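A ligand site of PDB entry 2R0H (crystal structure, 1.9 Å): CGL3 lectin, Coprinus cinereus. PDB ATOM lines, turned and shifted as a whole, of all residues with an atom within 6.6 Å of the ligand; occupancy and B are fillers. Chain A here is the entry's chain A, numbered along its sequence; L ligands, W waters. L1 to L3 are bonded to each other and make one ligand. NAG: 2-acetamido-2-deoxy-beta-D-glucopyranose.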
ATOM      1  N   THR A  41     -15.199  -0.683   7.306  1.00  0.00           N
ATOM      2  CA  THR A  41     -15.153  -2.147   7.543  1.00  0.00           C
ATOM      3  C   THR A  41     -16.244  -2.945   6.823  1.00  0.00           C
ATOM      4  O   THR A  41     -16.137  -4.172   6.647  1.00  0.00           O
ATOM      5  CB  THR A  41     -15.252  -2.502   9.053  1.00  0.00           C
ATOM      6  OG1 THR A  41     -16.546  -2.134   9.564  1.00  0.00           O
ATOM      7  CG2 THR A  41     -14.149  -1.851   9.852  1.00  0.00           C
ATOM      8  N   ILE A  43     -18.944  -3.841   7.965  1.00  0.00           N
ATOM      9  CA  ILE A  43     -19.694  -4.673   8.935  1.00  0.00           C
ATOM     10  C   ILE A  43     -20.161  -3.865  10.166  1.00  0.00           C
ATOM     11  O   ILE A  43     -19.317  -3.325  10.868  1.00  0.00           O
ATOM     12  CB  ILE A  43     -18.786  -5.811   9.461  1.00  0.00           C
ATOM     13  CG1 ILE A  43     -18.223  -6.638   8.297  1.00  0.00           C
ATOM     14  CG2 ILE A  43     -19.546  -6.659  10.453  1.00  0.00           C
ATOM     15  CD1 ILE A  43     -17.292  -7.773   8.735  1.00  0.00           C
ATOM     16  N   ASP A  44     -21.477  -3.735  10.365  1.00  0.00           N
ATOM     17  CA  ASP A  44     -22.069  -2.984  11.521  1.00  0.00           C
ATOM     18  C   ASP A  44     -21.804  -3.912  12.732  1.00  0.00           C
ATOM     19  O   ASP A  44     -22.495  -4.888  12.974  1.00  0.00           O
ATOM     20  CB  ASP A  44     -23.544  -2.699  11.265  1.00  0.00           C
ATOM     21  CG  ASP A  44     -24.203  -1.832  12.332  1.00  0.00           C
ATOM     22  OD1 ASP A  44     -25.218  -1.220  11.972  1.00  0.00           O
ATOM     23  OD2 ASP A  44     -23.701  -1.694  13.476  1.00  0.00           O
ATOM     24  N   ASN A  45     -20.809  -3.536  13.519  1.00  0.00           N
ATOM     25  CA  ASN A  45     -20.415  -4.369  14.643  1.00  0.00           C
ATOM     26  C   ASN A  45     -19.982  -3.643  15.918  1.00  0.00           C
ATOM     27  O   ASN A  45     -19.056  -2.837  15.884  1.00  0.00           O
ATOM     28  CB  ASN A  45     -19.228  -5.204  14.137  1.00  0.00           C
ATOM     29  CG  ASN A  45     -18.546  -6.000  15.231  1.00  0.00           C
ATOM     30  OD1 ASN A  45     -19.052  -6.097  16.325  1.00  0.00           O
ATOM     31  ND2 ASN A  45     -17.376  -6.547  14.935  1.00  0.00           N
ATOM     32  N   ASN A  47     -19.425  -4.619  19.989  1.00  0.00           N
ATOM     33  CA  ASN A  47     -19.222  -5.805  20.795  1.00  0.00           C
ATOM     34  C   ASN A  47     -18.682  -5.563  22.205  1.00  0.00           C
ATOM     35  O   ASN A  47     -18.080  -4.528  22.477  1.00  0.00           O
ATOM     36  CB  ASN A  47     -18.307  -6.794  20.068  1.00  0.00           C
ATOM     37  CG  ASN A  47     -17.017  -6.154  19.588  1.00  0.00           C
ATOM     38  OD1 ASN A  47     -17.008  -5.442  18.581  1.00  0.00           O
ATOM     39  ND2 ASN A  47     -15.934  -6.406  20.298  1.00  0.00           N
ATOM     40  N   ASN A  49     -16.567  -7.871  25.372  1.00  0.00           N
ATOM     41  CA  ASN A  49     -15.755  -9.074  25.370  1.00  0.00           C
ATOM     42  C   ASN A  49     -15.222  -9.342  26.756  1.00  0.00           C
ATOM     43  O   ASN A  49     -15.013  -8.403  27.514  1.00  0.00           O
ATOM     44  CB  ASN A  49     -14.483  -8.709  24.575  1.00  0.00           C
ATOM     45  CG  ASN A  49     -14.733  -8.268  23.139  1.00  0.00           C
ATOM     46  OD1 ASN A  49     -14.790  -7.062  22.835  1.00  0.00           O
ATOM     47  ND2 ASN A  49     -14.995  -9.233  22.269  1.00  0.00           N
ATOM     48  N   HIS A  60     -16.644 -13.244  23.109  1.00  0.00           N
ATOM     49  CA  HIS A  60     -16.904 -12.054  22.308  1.00  0.00           C
ATOM     50  C   HIS A  60     -18.407 -12.080  22.079  1.00  0.00           C
ATOM     51  O   HIS A  60     -18.936 -13.138  21.725  1.00  0.00           O
ATOM     52  CB  HIS A  60     -16.189 -12.123  20.962  1.00  0.00           C
ATOM     53  CG  HIS A  60     -16.583 -11.049  19.980  1.00  0.00           C
ATOM     54  ND1 HIS A  60     -17.591 -11.225  19.066  1.00  0.00           N
ATOM     55  CD2 HIS A  60     -16.041  -9.839  19.700  1.00  0.00           C
ATOM     56  CE1 HIS A  60     -17.685 -10.155  18.286  1.00  0.00           C
ATOM     57  NE2 HIS A  60     -16.730  -9.314  18.640  1.00  0.00           N
ATOM     58  N   ARG A  64     -25.087  -7.448  15.657  1.00  0.00           N
ATOM     59  CA  ARG A  64     -25.048  -7.143  14.241  1.00  0.00           C
ATOM     60  C   ARG A  64     -26.402  -6.698  13.738  1.00  0.00           C
ATOM     61  O   ARG A  64     -27.219  -7.533  13.350  1.00  0.00           O
ATOM     62  CB  ARG A  64     -24.602  -8.364  13.452  1.00  0.00           C
ATOM     63  CG  ARG A  64     -23.188  -8.906  13.808  1.00  0.00           C
ATOM     64  CD  ARG A  64     -22.060  -7.944  13.506  1.00  0.00           C
ATOM     65  NE  ARG A  64     -20.815  -8.604  13.918  1.00  0.00           N
ATOM     66  CZ  ARG A  64     -20.128  -9.416  13.117  1.00  0.00           C
ATOM     67  NH1 ARG A  64     -20.589  -9.651  11.873  1.00  0.00           N
ATOM     68  NH2 ARG A  64     -19.037 -10.008  13.542  1.00  0.00           N
ATOM     69  N   GLU A  67     -27.351  -7.636  10.180  1.00  0.00           N
ATOM     70  CA  GLU A  67     -27.371  -9.056   9.929  1.00  0.00           C
ATOM     71  C   GLU A  67     -28.426  -9.745  10.760  1.00  0.00           C
ATOM     72  O   GLU A  67     -28.639 -10.934  10.585  1.00  0.00           O
ATOM     73  CB  GLU A  67     -25.989  -9.652  10.290  1.00  0.00           C
ATOM     74  CG  GLU A  67     -24.796  -8.940   9.644  1.00  0.00           C
ATOM     75  CD  GLU A  67     -23.442  -9.504  10.086  1.00  0.00           C
ATOM     76  OE1 GLU A  67     -23.302 -10.735  10.212  1.00  0.00           O
ATOM     77  OE2 GLU A  67     -22.467  -8.722  10.193  1.00  0.00           O
ATOM     78  N   VAL A  71     -23.392 -12.477  17.528  1.00  0.00           N
ATOM     79  CA  VAL A  71     -22.304 -13.323  17.098  1.00  0.00           C
ATOM     80  C   VAL A  71     -21.517 -13.631  18.345  1.00  0.00           C
ATOM     81  O   VAL A  71     -21.125 -12.695  19.045  1.00  0.00           O
ATOM     82  CB  VAL A  71     -21.329 -12.635  16.123  1.00  0.00           C
ATOM     83  CG1 VAL A  71     -20.062 -13.547  15.891  1.00  0.00           C
ATOM     84  CG2 VAL A  71     -22.048 -12.323  14.828  1.00  0.00           C
ATOM     85  N   PHE A  72     -21.338 -14.909  18.654  1.00  0.00           N
ATOM     86  CA  PHE A  72     -20.551 -15.291  19.833  1.00  0.00           C
ATOM     87  C   PHE A  72     -19.270 -15.971  19.345  1.00  0.00           C
ATOM     88  O   PHE A  72     -19.318 -16.764  18.411  1.00  0.00           O
ATOM     89  CB  PHE A  72     -21.377 -16.241  20.710  1.00  0.00           C
ATOM     90  CG  PHE A  72     -22.686 -15.668  21.115  1.00  0.00           C
ATOM     91  CD1 PHE A  72     -22.736 -14.619  22.030  1.00  0.00           C
ATOM     92  CD2 PHE A  72     -23.879 -16.226  20.708  1.00  0.00           C
ATOM     93  CE1 PHE A  72     -23.926 -14.046  22.415  1.00  0.00           C
ATOM     94  CE2 PHE A  72     -25.102 -15.683  21.140  1.00  0.00           C
ATOM     95  CZ  PHE A  72     -25.110 -14.590  21.985  1.00  0.00           C
ATOM     96  N   ASN A  73     -18.119 -15.713  19.970  1.00  0.00           N
ATOM     97  CA  ASN A  73     -16.930 -16.365  19.486  1.00  0.00           C
ATOM     98  C   ASN A  73     -15.851 -16.174  20.559  1.00  0.00           C
ATOM     99  O   ASN A  73     -16.126 -15.627  21.630  1.00  0.00           O
ATOM    100  CB  ASN A  73     -16.543 -15.701  18.173  1.00  0.00           C
ATOM    101  CG  ASN A  73     -15.638 -16.560  17.292  1.00  0.00           C
ATOM    102  OD1 ASN A  73     -14.996 -17.545  17.710  1.00  0.00           O
ATOM    103  ND2 ASN A  73     -15.617 -16.205  16.019  1.00  0.00           N
ATOM    104  N   SER A  74     -14.692 -16.772  20.315  1.00  0.00           N
ATOM    105  CA  SER A  74     -13.532 -16.692  21.214  1.00  0.00           C
ATOM    106  C   SER A  74     -12.374 -16.346  20.292  1.00  0.00           C
ATOM    107  O   SER A  74     -12.271 -16.893  19.182  1.00  0.00           O
ATOM    108  CB  SER A  74     -13.275 -18.018  21.924  1.00  0.00           C
ATOM    109  OG  SER A  74     -14.377 -18.390  22.727  1.00  0.00           O
ATOM    110  N   ILE A  75     -11.514 -15.431  20.717  1.00  0.00           N
ATOM    111  CA  ILE A  75     -10.405 -15.058  19.882  1.00  0.00           C
ATOM    112  C   ILE A  75      -9.079 -15.045  20.620  1.00  0.00           C
ATOM    113  O   ILE A  75      -8.833 -14.162  21.448  1.00  0.00           O
ATOM    114  CB  ILE A  75     -10.549 -13.658  19.252  1.00  0.00           C
ATOM    115  CG1 ILE A  75     -11.897 -13.464  18.523  1.00  0.00           C
ATOM    116  CG2 ILE A  75      -9.391 -13.362  18.316  1.00  0.00           C
ATOM    117  CD1 ILE A  75     -13.043 -13.327  19.435  1.00  0.00           C
ATOM    118  N   ARG A  81     -10.232 -15.295  14.618  1.00  0.00           N
ATOM    119  CA  ARG A  81     -11.418 -15.788  15.268  1.00  0.00           C
ATOM    120  C   ARG A  81     -11.644 -17.286  15.054  1.00  0.00           C
ATOM    121  O   ARG A  81     -11.119 -17.873  14.113  1.00  0.00           O
ATOM    122  CB  ARG A  81     -12.639 -15.091  14.656  1.00  0.00           C
ATOM    123  CG  ARG A  81     -12.843 -15.369  13.199  1.00  0.00           C
ATOM    124  CD  ARG A  81     -14.149 -14.741  12.810  1.00  0.00           C
ATOM    125  NE  ARG A  81     -14.550 -14.866  11.404  1.00  0.00           N
ATOM    126  CZ  ARG A  81     -15.247 -15.883  10.930  1.00  0.00           C
ATOM    127  NH1 ARG A  81     -15.487 -16.949  11.692  1.00  0.00           N
ATOM    128  NH2 ARG A  81     -15.627 -15.882   9.662  1.00  0.00           N
ATOM    129  N   GLY A  82     -12.417 -17.900  15.942  1.00  0.00           N
ATOM    130  CA  GLY A  82     -12.825 -19.289  15.793  1.00  0.00           C
ATOM    131  C   GLY A  82     -14.094 -19.309  14.967  1.00  0.00           C
ATOM    132  O   GLY A  82     -14.432 -18.294  14.359  1.00  0.00           O
ATOM    133  N   PRO A  83     -14.818 -20.425  14.948  1.00  0.00           N
ATOM    134  CA  PRO A  83     -16.070 -20.421  14.181  1.00  0.00           C
ATOM    135  C   PRO A  83     -17.106 -19.589  14.959  1.00  0.00           C
ATOM    136  O   PRO A  83     -17.065 -19.556  16.182  1.00  0.00           O
ATOM    137  CB  PRO A  83     -16.474 -21.889  14.180  1.00  0.00           C
ATOM    138  CG  PRO A  83     -15.793 -22.478  15.393  1.00  0.00           C
ATOM    139  CD  PRO A  83     -14.520 -21.729  15.556  1.00  0.00           C
ATOM    140  N   GLU A  84     -18.000 -18.897  14.253  1.00  0.00           N
ATOM    141  CA  GLU A  84     -19.002 -18.078  14.939  1.00  0.00           C
ATOM    142  C   GLU A  84     -20.223 -18.854  15.350  1.00  0.00           C
ATOM    143  O   GLU A  84     -20.598 -19.814  14.695  1.00  0.00           O
ATOM    144  CB  GLU A  84     -19.472 -16.923  14.012  1.00  0.00           C
ATOM    145  CG  GLU A  84     -18.412 -15.920  13.689  1.00  0.00           C
ATOM    146  CD  GLU A  84     -18.867 -14.780  12.768  1.00  0.00           C
ATOM    147  OE1 GLU A  84     -18.147 -13.778  12.801  1.00  0.00           O
ATOM    148  OE2 GLU A  84     -19.910 -14.859  12.067  1.00  0.00           O
ATOM    149  N   ARG A  86     -24.104 -18.066  16.115  1.00  0.00           N
ATOM    150  CA  ARG A  86     -25.045 -16.966  15.956  1.00  0.00           C
ATOM    151  C   ARG A  86     -26.480 -17.299  16.340  1.00  0.00           C
ATOM    152  O   ARG A  86     -26.911 -18.446  16.214  1.00  0.00           O
ATOM    153  CB  ARG A  86     -24.979 -16.422  14.530  1.00  0.00           C
ATOM    154  CG  ARG A  86     -23.579 -15.999  14.100  1.00  0.00           C
ATOM    155  CD  ARG A  86     -23.473 -15.893  12.591  1.00  0.00           C
ATOM    156  NE  ARG A  86     -24.192 -14.740  12.059  1.00  0.00           N
ATOM    157  CZ  ARG A  86     -23.611 -13.639  11.616  1.00  0.00           C
ATOM    158  NH1 ARG A  86     -22.291 -13.517  11.630  1.00  0.00           N
ATOM    159  NH2 ARG A  86     -24.352 -12.644  11.151  1.00  0.00           N
ATOM    160  N   ASN A 138     -16.755  -1.026  15.333  1.00  0.00           N
ATOM    161  CA  ASN A 138     -16.051  -0.836  14.080  1.00  0.00           C
ATOM    162  C   ASN A 138     -15.931   0.655  13.772  1.00  0.00           C
ATOM    163  O   ASN A 138     -16.833   1.437  14.089  1.00  0.00           O
ATOM    164  CB  ASN A 138     -16.642  -1.648  12.922  1.00  0.00           C
ATOM    165  CG  ASN A 138     -16.330  -3.118  13.028  1.00  0.00           C
ATOM    166  OD1 ASN A 138     -15.647  -3.557  13.961  1.00  0.00           O
ATOM    167  ND2 ASN A 138     -16.743  -3.881  12.035  1.00  0.00           N
HETATM  168  C1  NAG L   1     -16.219 -14.939   3.539  1.00  0.00           C
HETATM  169  C2  NAG L   1     -15.006 -15.048   4.463  1.00  0.00           C
HETATM  170  C3  NAG L   1     -15.481 -14.967   5.914  1.00  0.00           C
HETATM  171  C4  NAG L   1     -16.367 -13.742   6.133  1.00  0.00           C
HETATM  172  C5  NAG L   1     -17.434 -13.571   5.052  1.00  0.00           C
HETATM  173  C6  NAG L   1     -18.024 -12.156   5.157  1.00  0.00           C
HETATM  174  C7  NAG L   1     -13.038 -16.463   4.028  1.00  0.00           C
HETATM  175  C8  NAG L   1     -12.359 -15.270   3.463  1.00  0.00           C
HETATM  176  N2  NAG L   1     -14.345 -16.328   4.235  1.00  0.00           N
HETATM  177  O1  NAG L   1     -15.810 -14.976   2.160  1.00  0.00           O
HETATM  178  O3  NAG L   1     -14.368 -14.934   6.843  1.00  0.00           O
HETATM  179  O4  NAG L   1     -17.035 -13.850   7.392  1.00  0.00           O
HETATM  180  O5  NAG L   1     -16.838 -13.676   3.765  1.00  0.00           O
HETATM  181  O6  NAG L   1     -19.435 -12.244   4.900  1.00  0.00           O
HETATM  182  O7  NAG L   1     -12.416 -17.495   4.272  1.00  0.00           O
HETATM  183  C1  NAG L   2     -16.965 -12.637   8.143  1.00  0.00           C
HETATM  184  C2  NAG L   2     -18.026 -12.721   9.235  1.00  0.00           C
HETATM  185  C3  NAG L   2     -17.851 -11.558  10.234  1.00  0.00           C
HETATM  186  C4  NAG L   2     -16.402 -11.434  10.711  1.00  0.00           C
HETATM  187  C5  NAG L   2     -15.440 -11.372   9.498  1.00  0.00           C
HETATM  188  C6  NAG L   2     -13.963 -11.301   9.872  1.00  0.00           C
HETATM  189  C7  NAG L   2     -20.110 -13.816   8.395  1.00  0.00           C
HETATM  190  C8  NAG L   2     -19.430 -15.130   8.532  1.00  0.00           C
HETATM  191  N2  NAG L   2     -19.393 -12.712   8.673  1.00  0.00           N
HETATM  192  O3  NAG L   2     -18.751 -11.795  11.305  1.00  0.00           O
HETATM  193  O4  NAG L   2     -16.298 -10.239  11.483  1.00  0.00           O
HETATM  194  O5  NAG L   2     -15.642 -12.551   8.711  1.00  0.00           O
HETATM  195  O6  NAG L   2     -13.642 -12.505  10.574  1.00  0.00           O
HETATM  196  O7  NAG L   2     -21.277 -13.746   8.025  1.00  0.00           O
HETATM  197  C1  NAG L   3     -15.541 -10.372  12.687  1.00  0.00           C
HETATM  198  C2  NAG L   3     -15.369  -8.997  13.310  1.00  0.00           C
HETATM  199  C3  NAG L   3     -14.526  -9.104  14.587  1.00  0.00           C
HETATM  200  C4  NAG L   3     -15.126 -10.173  15.513  1.00  0.00           C
HETATM  201  C5  NAG L   3     -15.428 -11.483  14.794  1.00  0.00           C
HETATM  202  C6  NAG L   3     -16.246 -12.392  15.693  1.00  0.00           C
HETATM  203  C7  NAG L   3     -15.159  -6.968  11.951  1.00  0.00           C
HETATM  204  C8  NAG L   3     -14.132  -6.154  11.209  1.00  0.00           C
HETATM  205  N2  NAG L   3     -14.714  -8.170  12.312  1.00  0.00           N
HETATM  206  O3  NAG L   3     -14.654  -7.861  15.297  1.00  0.00           O
HETATM  207  O4  NAG L   3     -14.269 -10.401  16.644  1.00  0.00           O
HETATM  208  O5  NAG L   3     -16.218 -11.201  13.629  1.00  0.00           O
HETATM  209  O6  NAG L   3     -16.693 -13.506  14.932  1.00  0.00           O
HETATM  210  O7  NAG L   3     -16.310  -6.596  12.167  1.00  0.00           O
HETATM  211  O   HOH W   1     -20.368 -10.143   8.575  1.00  0.00           O
HETATM  212  O   HOH W   2     -11.915 -13.667   8.076  1.00  0.00           O
HETATM  213  O   HOH W   3     -11.907  -9.072  11.864  1.00  0.00           O
HETATM  214  O   HOH W   4     -16.172 -18.531   4.701  1.00  0.00           O
HETATM  215  O   HOH W   5     -13.641  -5.297  14.258  1.00  0.00           O
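An oxygen (O3) of NAG L2 is in hydrogen-bond range of the side-chain carboxylate (OE1) of Glu 84 (2.6 Å).
An oxygen (O6) of NAG L2 sits at hydrogen-bond distance from the guanidinium group of Arg 81, at 2.7 Å.
ND2 of Asn 138 sits at hydrogen-bond distance from O7 of NAG L3, 2.8 Å away.
The guanidinium group of Arg 64 is in hydrogen-bond range of an oxygen (O3) of NAG L2 (2.9 Å).
ND2 of Asn 45 is in hydrogen-bond range of O7 of NAG L3 (3.0 Å).
The side-chain amide nitrogen of Asn 73 sits at hydrogen-bond distance from an oxygen (O6) of NAG L3 (3.1 Å).
A ring nitrogen (NE2) of His 60 is in hydrogen-bond range of an oxygen (O4) of NAG L3 (3.3 Å).
The guanidinium group (NH1) of Arg 86 lies within salt-bridge range of the side-chain carboxylate (OE2) of Glu 84.
The side-chain amide nitrogen of Asn 138 is in hydrogen-bond range of the backbone carbonyl oxygen of Ile 43, 2.9 Å away.
The side-chain amide nitrogen (ND2) of Asn 138 sits at hydrogen-bond distance from the side-chain hydroxyl (OG1) of Thr 41 (3.0 Å).
O of Asn 73 lies within hydrogen-bond range of N of His 60 (2.9 Å).
The backbone carbonyl oxygen (O) of Pro 83 lies close to the side-chain amide oxygen (OD1) of Asn 73 (3.3 Å).
The side-chain amide nitrogen (ND2) of Asn 47 lies close to a ring nitrogen (NE2) of His 60 (3.4 Å).
The backbone carbonyl oxygen (O) of Ile 43 is in hydrogen-bond range of the side-chain hydroxyl (OG1) of Thr 41 (3.3 Å).
NH1 of Arg 86 is in salt-bridge range of OE1 of Glu 67.
Ile 43 touches the ligand.
CG1 of Val 71 touches O6 of NAG L3, at 3.5 Å.
NH1 of Arg 86 touches O7 of NAG L2, at 3.8 Å.
Hydrophobic or aromatic side chains that line the ligand: Ile 43, His 60 and Val 71.
The nearest printed residue that does not touch the ligand is Ile 75 (4.2 Å).
Water W1 lies within hydrogen-bond range of N2 of NAG L2, OE2 of Glu 67 and NH1 of Arg 64.
Water W5 bridges OD1 of Asn 138 and O3 of NAG L3.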
